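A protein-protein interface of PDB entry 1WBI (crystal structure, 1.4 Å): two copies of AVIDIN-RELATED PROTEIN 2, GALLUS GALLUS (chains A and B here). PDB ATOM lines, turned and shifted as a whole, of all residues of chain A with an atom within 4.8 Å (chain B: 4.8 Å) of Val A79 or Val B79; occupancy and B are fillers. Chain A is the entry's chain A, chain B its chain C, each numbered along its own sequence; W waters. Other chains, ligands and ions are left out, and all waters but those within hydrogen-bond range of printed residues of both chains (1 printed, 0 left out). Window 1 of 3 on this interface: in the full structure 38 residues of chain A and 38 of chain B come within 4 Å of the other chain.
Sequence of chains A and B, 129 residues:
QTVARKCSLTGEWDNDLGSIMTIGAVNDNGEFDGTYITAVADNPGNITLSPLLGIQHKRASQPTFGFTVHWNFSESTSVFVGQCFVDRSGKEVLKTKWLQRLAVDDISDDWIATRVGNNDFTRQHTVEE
Of chain B, only Gly B66 (3.9 Å), Val B79 (3.6 Å), Phe B80 (3.5 Å) and Val B81 (3.8 Å) come within 4 Å of Val A79.
Val B79 touches four residues of chain A.
Printed residues of chain A within 4 Å of Thr B77: Gly A66 and Val A81.
Of the printed residues of chain A, Leu B99 touches Val A81 (3.7 Å), Lys A97 (3.7 Å), Trp A98 (3.8 Å) and Leu A99 (3.7 Å).
Printed residues of chain B within 4 Å of Lys A97: Leu B99 (3.7 Å).
Of the printed residues of chain A, Phe B80 touches Val A79 (3.5 Å).
Ser B78 touches none of the printed residues of chain A.
Ser A78 touches none of the printed residues of chain B.
The nearest residue of chain B that does not touch Val A79 is Phe B67 (4.2 Å).
The nearest printed residue of chain A that does not touch Phe B80 is Thr A68 (5.1 Å).
Of the 11 printed residues of chain B, 10 touch a printed residue of chain A.
Hydrophobic or aromatic side chains of chain B that line the printed part of chain A: Val B79, Val B81 and Leu B99.
Of the 11 printed residues of chain A, 10 touch a printed residue of chain B.
Printed residues of chain A that touch a printed residue of chain B: Gly A66, Phe A67, Thr A68, Thr A77, Val A79, Phe A80, Val A81, Lys A97, Trp A98 and Leu A99.
Among the printed residues, 22 pairs touch across the chains.
Among the printed residues, no Asp or Glu carboxylate lies within 4 Å of a Lys or Arg side-chain nitrogen of the other chain.
The backbone carbonyl oxygen of Phe B67 is in hydrogen-bond range of the backbone NH of Phe B80.
The backbone NH (N) of Val B81 is in hydrogen-bond range of the backbone carbonyl oxygen (O) of Lys B97, 2.9 Å away.
The backbone carbonyl oxygen of Lys A97 lies within hydrogen-bond range of the backbone NH of Val A81, at 2.9 Å.
N of Phe A80 is in hydrogen-bond range of O of Phe A67 (2.9 Å).
The backbone carbonyl oxygen of Leu A99 sits at hydrogen-bond distance from the backbone NH of Val A79, 2.9 Å away.
O of Leu B99 sits at hydrogen-bond distance from N of Val B79 (2.9 Å).
Gly A66 touches Thr B77, and with the chains exchanged Thr A77 touches Gly B66.
Gly A66 touches Val B79, and with the chains exchanged Val A79 touches Gly B66.
Val A79 touches Val B81, and with the chains exchanged Val A81 touches Val B79.
Leu A99 touches its own counterpart, Leu B99.
N of Phe A67 sits at hydrogen-bond distance from OG1 of Thr B68, 3.3 Å away.
The side-chain hydroxyl (OG1) of Thr A68 sits close to the backbone carbonyl oxygen (O) of Gly B66, 3.4 Å away.
The side-chain hydroxyl (OG1) of Thr B68 sits close to the backbone carbonyl oxygen (O) of Gly A66, at 3.4 Å.
The backbone NH (N) of Phe B67 lies within hydrogen-bond range of the side-chain hydroxyl (OG1) of Thr A68 (3.4 Å).
Water W1 lies within hydrogen-bond range of OG1 of Thr A68 (2.8 Å) and OG1 of Thr B68 (2.8 Å).
N of Gly A66 touches CG2 of Thr B77, at 3.7 Å.
Val B79 touches Gly A66 (CG1 to CA, 3.9 Å).
Thr A77 touches Val B81 (O to CG2, 3.6 Å).
CG1 of Val A79 touches CA of Gly B66, 3.9 Å away.
Val A79 touches Phe B80.
Val A79 touches Val B81.
Val B79 touches Val A81.
Val A81 touches Leu B99.
N of Trp B98 touches CD1 of Leu A99, 3.8 Å away.
Leu B99 touches Leu A99.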
ATOM      1  N   GLY A  66       2.019  -8.121   8.279  1.00  0.00           N
ATOM      2  CA  GLY A  66       1.685  -9.059   9.331  1.00  0.00           C
ATOM      3  C   GLY A  66       1.918 -10.479   8.859  1.00  0.00           C
ATOM      4  O   GLY A  66       1.907 -10.744   7.622  1.00  0.00           O
ATOM      5  N   PHE A  67       2.160 -11.397   9.798  1.00  0.00           N
ATOM      6  CA  PHE A  67       2.171 -12.807   9.470  1.00  0.00           C
ATOM      7  C   PHE A  67       1.767 -13.677  10.633  1.00  0.00           C
ATOM      8  O   PHE A  67       1.850 -13.266  11.779  1.00  0.00           O
ATOM      9  CB  PHE A  67       3.521 -13.259   8.858  1.00  0.00           C
ATOM     10  CG  PHE A  67       4.721 -13.066   9.748  1.00  0.00           C
ATOM     11  CD1 PHE A  67       5.159 -14.061  10.584  1.00  0.00           C
ATOM     12  CD2 PHE A  67       5.472 -11.907   9.671  1.00  0.00           C
ATOM     13  CE1 PHE A  67       6.270 -13.888  11.389  1.00  0.00           C
ATOM     14  CE2 PHE A  67       6.582 -11.709  10.477  1.00  0.00           C
ATOM     15  CZ  PHE A  67       7.026 -12.736  11.304  1.00  0.00           C
ATOM     16  N   THR A  68       1.378 -14.900  10.289  1.00  0.00           N
ATOM     17  CA  THR A  68       0.979 -15.956  11.221  1.00  0.00           C
ATOM     18  C   THR A  68       2.018 -17.061  11.161  1.00  0.00           C
ATOM     19  O   THR A  68       2.469 -17.418  10.053  1.00  0.00           O
ATOM     20  CB  THR A  68      -0.377 -16.559  10.862  1.00  0.00           C
ATOM     21  OG1 THR A  68      -1.411 -15.539  10.926  1.00  0.00           O
ATOM     22  CG2 THR A  68      -0.774 -17.625  11.791  1.00  0.00           C
ATOM     23  N   THR A  77      -0.290 -20.899  18.177  1.00  0.00           N
ATOM     24  CA  THR A  77      -0.090 -20.103  16.987  1.00  0.00           C
ATOM     25  C   THR A  77       0.397 -18.736  17.446  1.00  0.00           C
ATOM     26  O   THR A  77      -0.051 -18.261  18.503  1.00  0.00           O
ATOM     27  CB  THR A  77      -1.425 -19.911  16.258  1.00  0.00           C
ATOM     28  OG1 THR A  77      -1.978 -21.219  15.923  1.00  0.00           O
ATOM     29  CG2 THR A  77      -1.270 -19.087  15.012  1.00  0.00           C
ATOM     30  N   SER A  78       1.298 -18.146  16.693  1.00  0.00           N
ATOM     31  CA  SER A  78       1.715 -16.754  16.937  1.00  0.00           C
ATOM     32  C   SER A  78       1.391 -15.877  15.738  1.00  0.00           C
ATOM     33  O   SER A  78       1.367 -16.350  14.629  1.00  0.00           O
ATOM     34  CB  SER A  78       3.201 -16.652  17.215  1.00  0.00           C
ATOM     35  OG  SER A  78       3.509 -17.283  18.465  1.00  0.00           O
ATOM     36  N   VAL A  79       1.143 -14.586  15.998  1.00  0.00           N
ATOM     37  CA  VAL A  79       1.047 -13.584  14.944  1.00  0.00           C
ATOM     38  C   VAL A  79       1.952 -12.415  15.264  1.00  0.00           C
ATOM     39  O   VAL A  79       2.192 -12.070  16.456  1.00  0.00           O
ATOM     40  CB  VAL A  79      -0.382 -13.059  14.754  1.00  0.00           C
ATOM     41  CG1 VAL A  79      -1.365 -14.165  14.266  1.00  0.00           C
ATOM     42  CG2 VAL A  79      -0.928 -12.489  16.063  1.00  0.00           C
ATOM     43  N   PHE A  80       2.544 -11.871  14.203  1.00  0.00           N
ATOM     44  CA  PHE A  80       3.442 -10.723  14.257  1.00  0.00           C
ATOM     45  C   PHE A  80       2.889  -9.621  13.386  1.00  0.00           C
ATOM     46  O   PHE A  80       2.438  -9.873  12.266  1.00  0.00           O
ATOM     47  CB  PHE A  80       4.833 -11.128  13.715  1.00  0.00           C
ATOM     48  CG  PHE A  80       5.609 -12.129  14.557  1.00  0.00           C
ATOM     49  CD1 PHE A  80       6.638 -11.706  15.339  1.00  0.00           C
ATOM     50  CD2 PHE A  80       5.259 -13.470  14.585  1.00  0.00           C
ATOM     51  CE1 PHE A  80       7.377 -12.643  16.109  1.00  0.00           C
ATOM     52  CE2 PHE A  80       5.994 -14.381  15.383  1.00  0.00           C
ATOM     53  CZ  PHE A  80       6.989 -13.942  16.131  1.00  0.00           C
ATOM     54  N   VAL A  81       2.983  -8.372  13.842  1.00  0.00           N
ATOM     55  CA  VAL A  81       2.589  -7.222  12.992  1.00  0.00           C
ATOM     56  C   VAL A  81       3.596  -6.130  13.177  1.00  0.00           C
ATOM     57  O   VAL A  81       4.148  -5.946  14.264  1.00  0.00           O
ATOM     58  CB  VAL A  81       1.179  -6.737  13.343  1.00  0.00           C
ATOM     59  CG1 VAL A  81       1.132  -5.938  14.624  1.00  0.00           C
ATOM     60  CG2 VAL A  81       0.567  -5.970  12.201  1.00  0.00           C
ATOM     61  N   LYS A  97       5.446  -6.261  16.920  1.00  0.00           N
ATOM     62  CA  LYS A  97       4.808  -6.730  18.132  1.00  0.00           C
ATOM     63  C   LYS A  97       4.104  -8.024  17.789  1.00  0.00           C
ATOM     64  O   LYS A  97       3.706  -8.253  16.638  1.00  0.00           O
ATOM     65  CB  LYS A  97       3.869  -5.687  18.719  1.00  0.00           C
ATOM     66  CG  LYS A  97       4.755  -4.547  19.283  1.00  0.00           C
ATOM     67  CD  LYS A  97       4.157  -3.283  19.692  1.00  0.00           C
ATOM     68  CE  LYS A  97       5.153  -2.259  20.231  1.00  0.00           C
ATOM     69  NZ  LYS A  97       6.477  -3.171  20.989  1.00  0.00           N
ATOM     70  N   TRP A  98       3.962  -8.891  18.781  1.00  0.00           N
ATOM     71  CA  TRP A  98       3.401 -10.208  18.575  1.00  0.00           C
ATOM     72  C   TRP A  98       2.467 -10.605  19.675  1.00  0.00           C
ATOM     73  O   TRP A  98       2.544 -10.102  20.818  1.00  0.00           O
ATOM     74  CB  TRP A  98       4.509 -11.290  18.365  1.00  0.00           C
ATOM     75  CG  TRP A  98       5.547 -11.422  19.447  1.00  0.00           C
ATOM     76  CD1 TRP A  98       6.827 -10.962  19.381  1.00  0.00           C
ATOM     77  CD2 TRP A  98       5.413 -12.066  20.717  1.00  0.00           C
ATOM     78  NE1 TRP A  98       7.498 -11.266  20.549  1.00  0.00           N
ATOM     79  CE2 TRP A  98       6.652 -11.969  21.370  1.00  0.00           C
ATOM     80  CE3 TRP A  98       4.386 -12.790  21.331  1.00  0.00           C
ATOM     81  CZ2 TRP A  98       6.861 -12.496  22.677  1.00  0.00           C
ATOM     82  CZ3 TRP A  98       4.594 -13.322  22.580  1.00  0.00           C
ATOM     83  CH2 TRP A  98       5.839 -13.179  23.252  1.00  0.00           C
ATOM     84  N   LEU A  99       1.604 -11.552  19.311  1.00  0.00           N
ATOM     85  CA  LEU A  99       0.733 -12.263  20.253  1.00  0.00           C
ATOM     86  C   LEU A  99       0.966 -13.777  20.024  1.00  0.00           C
ATOM     87  O   LEU A  99       1.018 -14.234  18.861  1.00  0.00           O
ATOM     88  CB  LEU A  99      -0.750 -11.952  20.006  1.00  0.00           C
ATOM     89  CG  LEU A  99      -1.188 -10.499  20.146  1.00  0.00           C
ATOM     90  CD1 LEU A  99      -2.640 -10.364  19.656  1.00  0.00           C
ATOM     91  CD2 LEU A  99      -1.102 -10.048  21.522  1.00  0.00           C
ATOM     92  N   GLY B  66      -4.471 -18.112  13.463  1.00  0.00           N
ATOM     93  CA  GLY B  66      -4.173 -16.689  13.317  1.00  0.00           C
ATOM     94  C   GLY B  66      -4.417 -16.263  11.875  1.00  0.00           C
ATOM     95  O   GLY B  66      -4.407 -17.079  10.934  1.00  0.00           O
ATOM     96  N   PHE B  67      -4.624 -14.954  11.699  1.00  0.00           N
ATOM     97  CA  PHE B  67      -4.654 -14.369  10.351  1.00  0.00           C
ATOM     98  C   PHE B  67      -4.244 -12.902  10.348  1.00  0.00           C
ATOM     99  O   PHE B  67      -4.269 -12.224  11.400  1.00  0.00           O
ATOM    100  CB  PHE B  67      -6.036 -14.554   9.638  1.00  0.00           C
ATOM    101  CG  PHE B  67      -7.220 -13.954  10.383  1.00  0.00           C
ATOM    102  CD1 PHE B  67      -7.631 -12.678  10.096  1.00  0.00           C
ATOM    103  CD2 PHE B  67      -7.961 -14.687  11.276  1.00  0.00           C
ATOM    104  CE1 PHE B  67      -8.692 -12.120  10.757  1.00  0.00           C
ATOM    105  CE2 PHE B  67      -9.062 -14.139  11.907  1.00  0.00           C
ATOM    106  CZ  PHE B  67      -9.418 -12.841  11.635  1.00  0.00           C
ATOM    107  N   THR B  68      -3.855 -12.475   9.165  1.00  0.00           N
ATOM    108  CA  THR B  68      -3.458 -11.118   8.878  1.00  0.00           C
ATOM    109  C   THR B  68      -4.519 -10.495   7.959  1.00  0.00           C
ATOM    110  O   THR B  68      -4.990 -11.181   7.026  1.00  0.00           O
ATOM    111  CB  THR B  68      -2.118 -11.088   8.096  1.00  0.00           C
ATOM    112  OG1 THR B  68      -1.061 -11.648   8.922  1.00  0.00           O
ATOM    113  CG2 THR B  68      -1.697  -9.704   7.751  1.00  0.00           C
ATOM    114  N   THR B  77      -2.101  -2.555   8.955  1.00  0.00           N
ATOM    115  CA  THR B  77      -2.299  -3.996   8.888  1.00  0.00           C
ATOM    116  C   THR B  77      -2.775  -4.442  10.277  1.00  0.00           C
ATOM    117  O   THR B  77      -2.288  -3.938  11.276  1.00  0.00           O
ATOM    118  CB  THR B  77      -0.977  -4.759   8.518  1.00  0.00           C
ATOM    119  OG1 THR B  77      -0.434  -4.285   7.260  1.00  0.00           O
ATOM    120  CG2 THR B  77      -1.158  -6.258   8.450  1.00  0.00           C
ATOM    121  N   SER B  78      -3.662  -5.436  10.330  1.00  0.00           N
ATOM    122  CA  SER B  78      -4.079  -6.042  11.590  1.00  0.00           C
ATOM    123  C   SER B  78      -3.775  -7.531  11.570  1.00  0.00           C
ATOM    124  O   SER B  78      -3.785  -8.157  10.521  1.00  0.00           O
ATOM    125  CB  SER B  78      -5.555  -5.807  11.929  1.00  0.00           C
ATOM    126  OG  SER B  78      -5.799  -4.424  12.141  1.00  0.00           O
ATOM    127  N   VAL B  79      -3.502  -8.064  12.775  1.00  0.00           N
ATOM    128  CA  VAL B  79      -3.385  -9.495  12.948  1.00  0.00           C
ATOM    129  C   VAL B  79      -4.327  -9.921  14.082  1.00  0.00           C
ATOM    130  O   VAL B  79      -4.512  -9.196  15.075  1.00  0.00           O
ATOM    131  CB  VAL B  79      -1.928  -9.942  13.258  1.00  0.00           C
ATOM    132  CG1 VAL B  79      -1.069  -9.723  12.045  1.00  0.00           C
ATOM    133  CG2 VAL B  79      -1.371  -9.280  14.528  1.00  0.00           C
ATOM    134  N   PHE B  80      -4.877 -11.118  13.914  1.00  0.00           N
ATOM    135  CA  PHE B  80      -5.790 -11.718  14.898  1.00  0.00           C
ATOM    136  C   PHE B  80      -5.249 -13.124  15.248  1.00  0.00           C
ATOM    137  O   PHE B  80      -4.843 -13.856  14.342  1.00  0.00           O
ATOM    138  CB  PHE B  80      -7.170 -11.886  14.286  1.00  0.00           C
ATOM    139  CG  PHE B  80      -7.937 -10.595  14.034  1.00  0.00           C
ATOM    140  CD1 PHE B  80      -8.972 -10.242  14.899  1.00  0.00           C
ATOM    141  CD2 PHE B  80      -7.635  -9.797  12.976  1.00  0.00           C
ATOM    142  CE1 PHE B  80      -9.730  -9.096  14.671  1.00  0.00           C
ATOM    143  CE2 PHE B  80      -8.370  -8.596  12.738  1.00  0.00           C
ATOM    144  CZ  PHE B  80      -9.410  -8.268  13.609  1.00  0.00           C
ATOM    145  N   VAL B  81      -5.338 -13.479  16.515  1.00  0.00           N
ATOM    146  CA  VAL B  81      -4.935 -14.827  16.966  1.00  0.00           C
ATOM    147  C   VAL B  81      -5.929 -15.298  17.982  1.00  0.00           C
ATOM    148  O   VAL B  81      -6.460 -14.506  18.765  1.00  0.00           O
ATOM    149  CB  VAL B  81      -3.469 -14.840  17.535  1.00  0.00           C
ATOM    150  CG1 VAL B  81      -3.389 -14.314  18.910  1.00  0.00           C
ATOM    151  CG2 VAL B  81      -2.889 -16.259  17.450  1.00  0.00           C
ATOM    152  N   LYS B  97      -7.692 -12.214  20.137  1.00  0.00           N
ATOM    153  CA  LYS B  97      -7.047 -10.929  20.434  1.00  0.00           C
ATOM    154  C   LYS B  97      -6.357 -10.468  19.156  1.00  0.00           C
ATOM    155  O   LYS B  97      -5.997 -11.278  18.316  1.00  0.00           O
ATOM    156  CB  LYS B  97      -6.087 -11.085  21.631  1.00  0.00           C
ATOM    157  CG  LYS B  97      -6.936 -11.341  22.899  1.00  0.00           C
ATOM    158  CD  LYS B  97      -6.300 -11.660  24.155  1.00  0.00           C
ATOM    159  CE  LYS B  97      -7.342 -11.722  25.264  1.00  0.00           C
ATOM    160  NZ  LYS B  97      -6.793 -12.376  26.510  1.00  0.00           N
ATOM    161  N   TRP B  98      -6.174  -9.154  19.053  1.00  0.00           N
ATOM    162  CA  TRP B  98      -5.617  -8.592  17.874  1.00  0.00           C
ATOM    163  C   TRP B  98      -4.640  -7.471  18.192  1.00  0.00           C
ATOM    164  O   TRP B  98      -4.663  -6.880  19.281  1.00  0.00           O
ATOM    165  CB  TRP B  98      -6.756  -8.072  16.945  1.00  0.00           C
ATOM    166  CG  TRP B  98      -7.753  -7.085  17.533  1.00  0.00           C
ATOM    167  CD1 TRP B  98      -9.029  -7.364  17.928  1.00  0.00           C
ATOM    168  CD2 TRP B  98      -7.541  -5.694  17.768  1.00  0.00           C
ATOM    169  NE1 TRP B  98      -9.642  -6.212  18.352  1.00  0.00           N
ATOM    170  CE2 TRP B  98      -8.760  -5.163  18.261  1.00  0.00           C
ATOM    171  CE3 TRP B  98      -6.492  -4.812  17.497  1.00  0.00           C
ATOM    172  CZ2 TRP B  98      -8.894  -3.799  18.593  1.00  0.00           C
ATOM    173  CZ3 TRP B  98      -6.659  -3.454  17.806  1.00  0.00           C
ATOM    174  CH2 TRP B  98      -7.834  -2.977  18.345  1.00  0.00           C
ATOM    175  N   LEU B  99      -3.819  -7.214  17.192  1.00  0.00           N
ATOM    176  CA  LEU B  99      -2.952  -6.024  17.154  1.00  0.00           C
ATOM    177  C   LEU B  99      -3.232  -5.310  15.823  1.00  0.00           C
ATOM    178  O   LEU B  99      -3.312  -5.942  14.770  1.00  0.00           O
ATOM    179  CB  LEU B  99      -1.472  -6.425  17.215  1.00  0.00           C
ATOM    180  CG  LEU B  99      -0.998  -7.122  18.508  1.00  0.00           C
ATOM    181  CD1 LEU B  99       0.409  -7.713  18.271  1.00  0.00           C
ATOM    182  CD2 LEU B  99      -1.021  -6.222  19.672  1.00  0.00           C
HETATM  183  O   HOH W   1      -1.267 -14.409   8.354  1.00  0.00           O
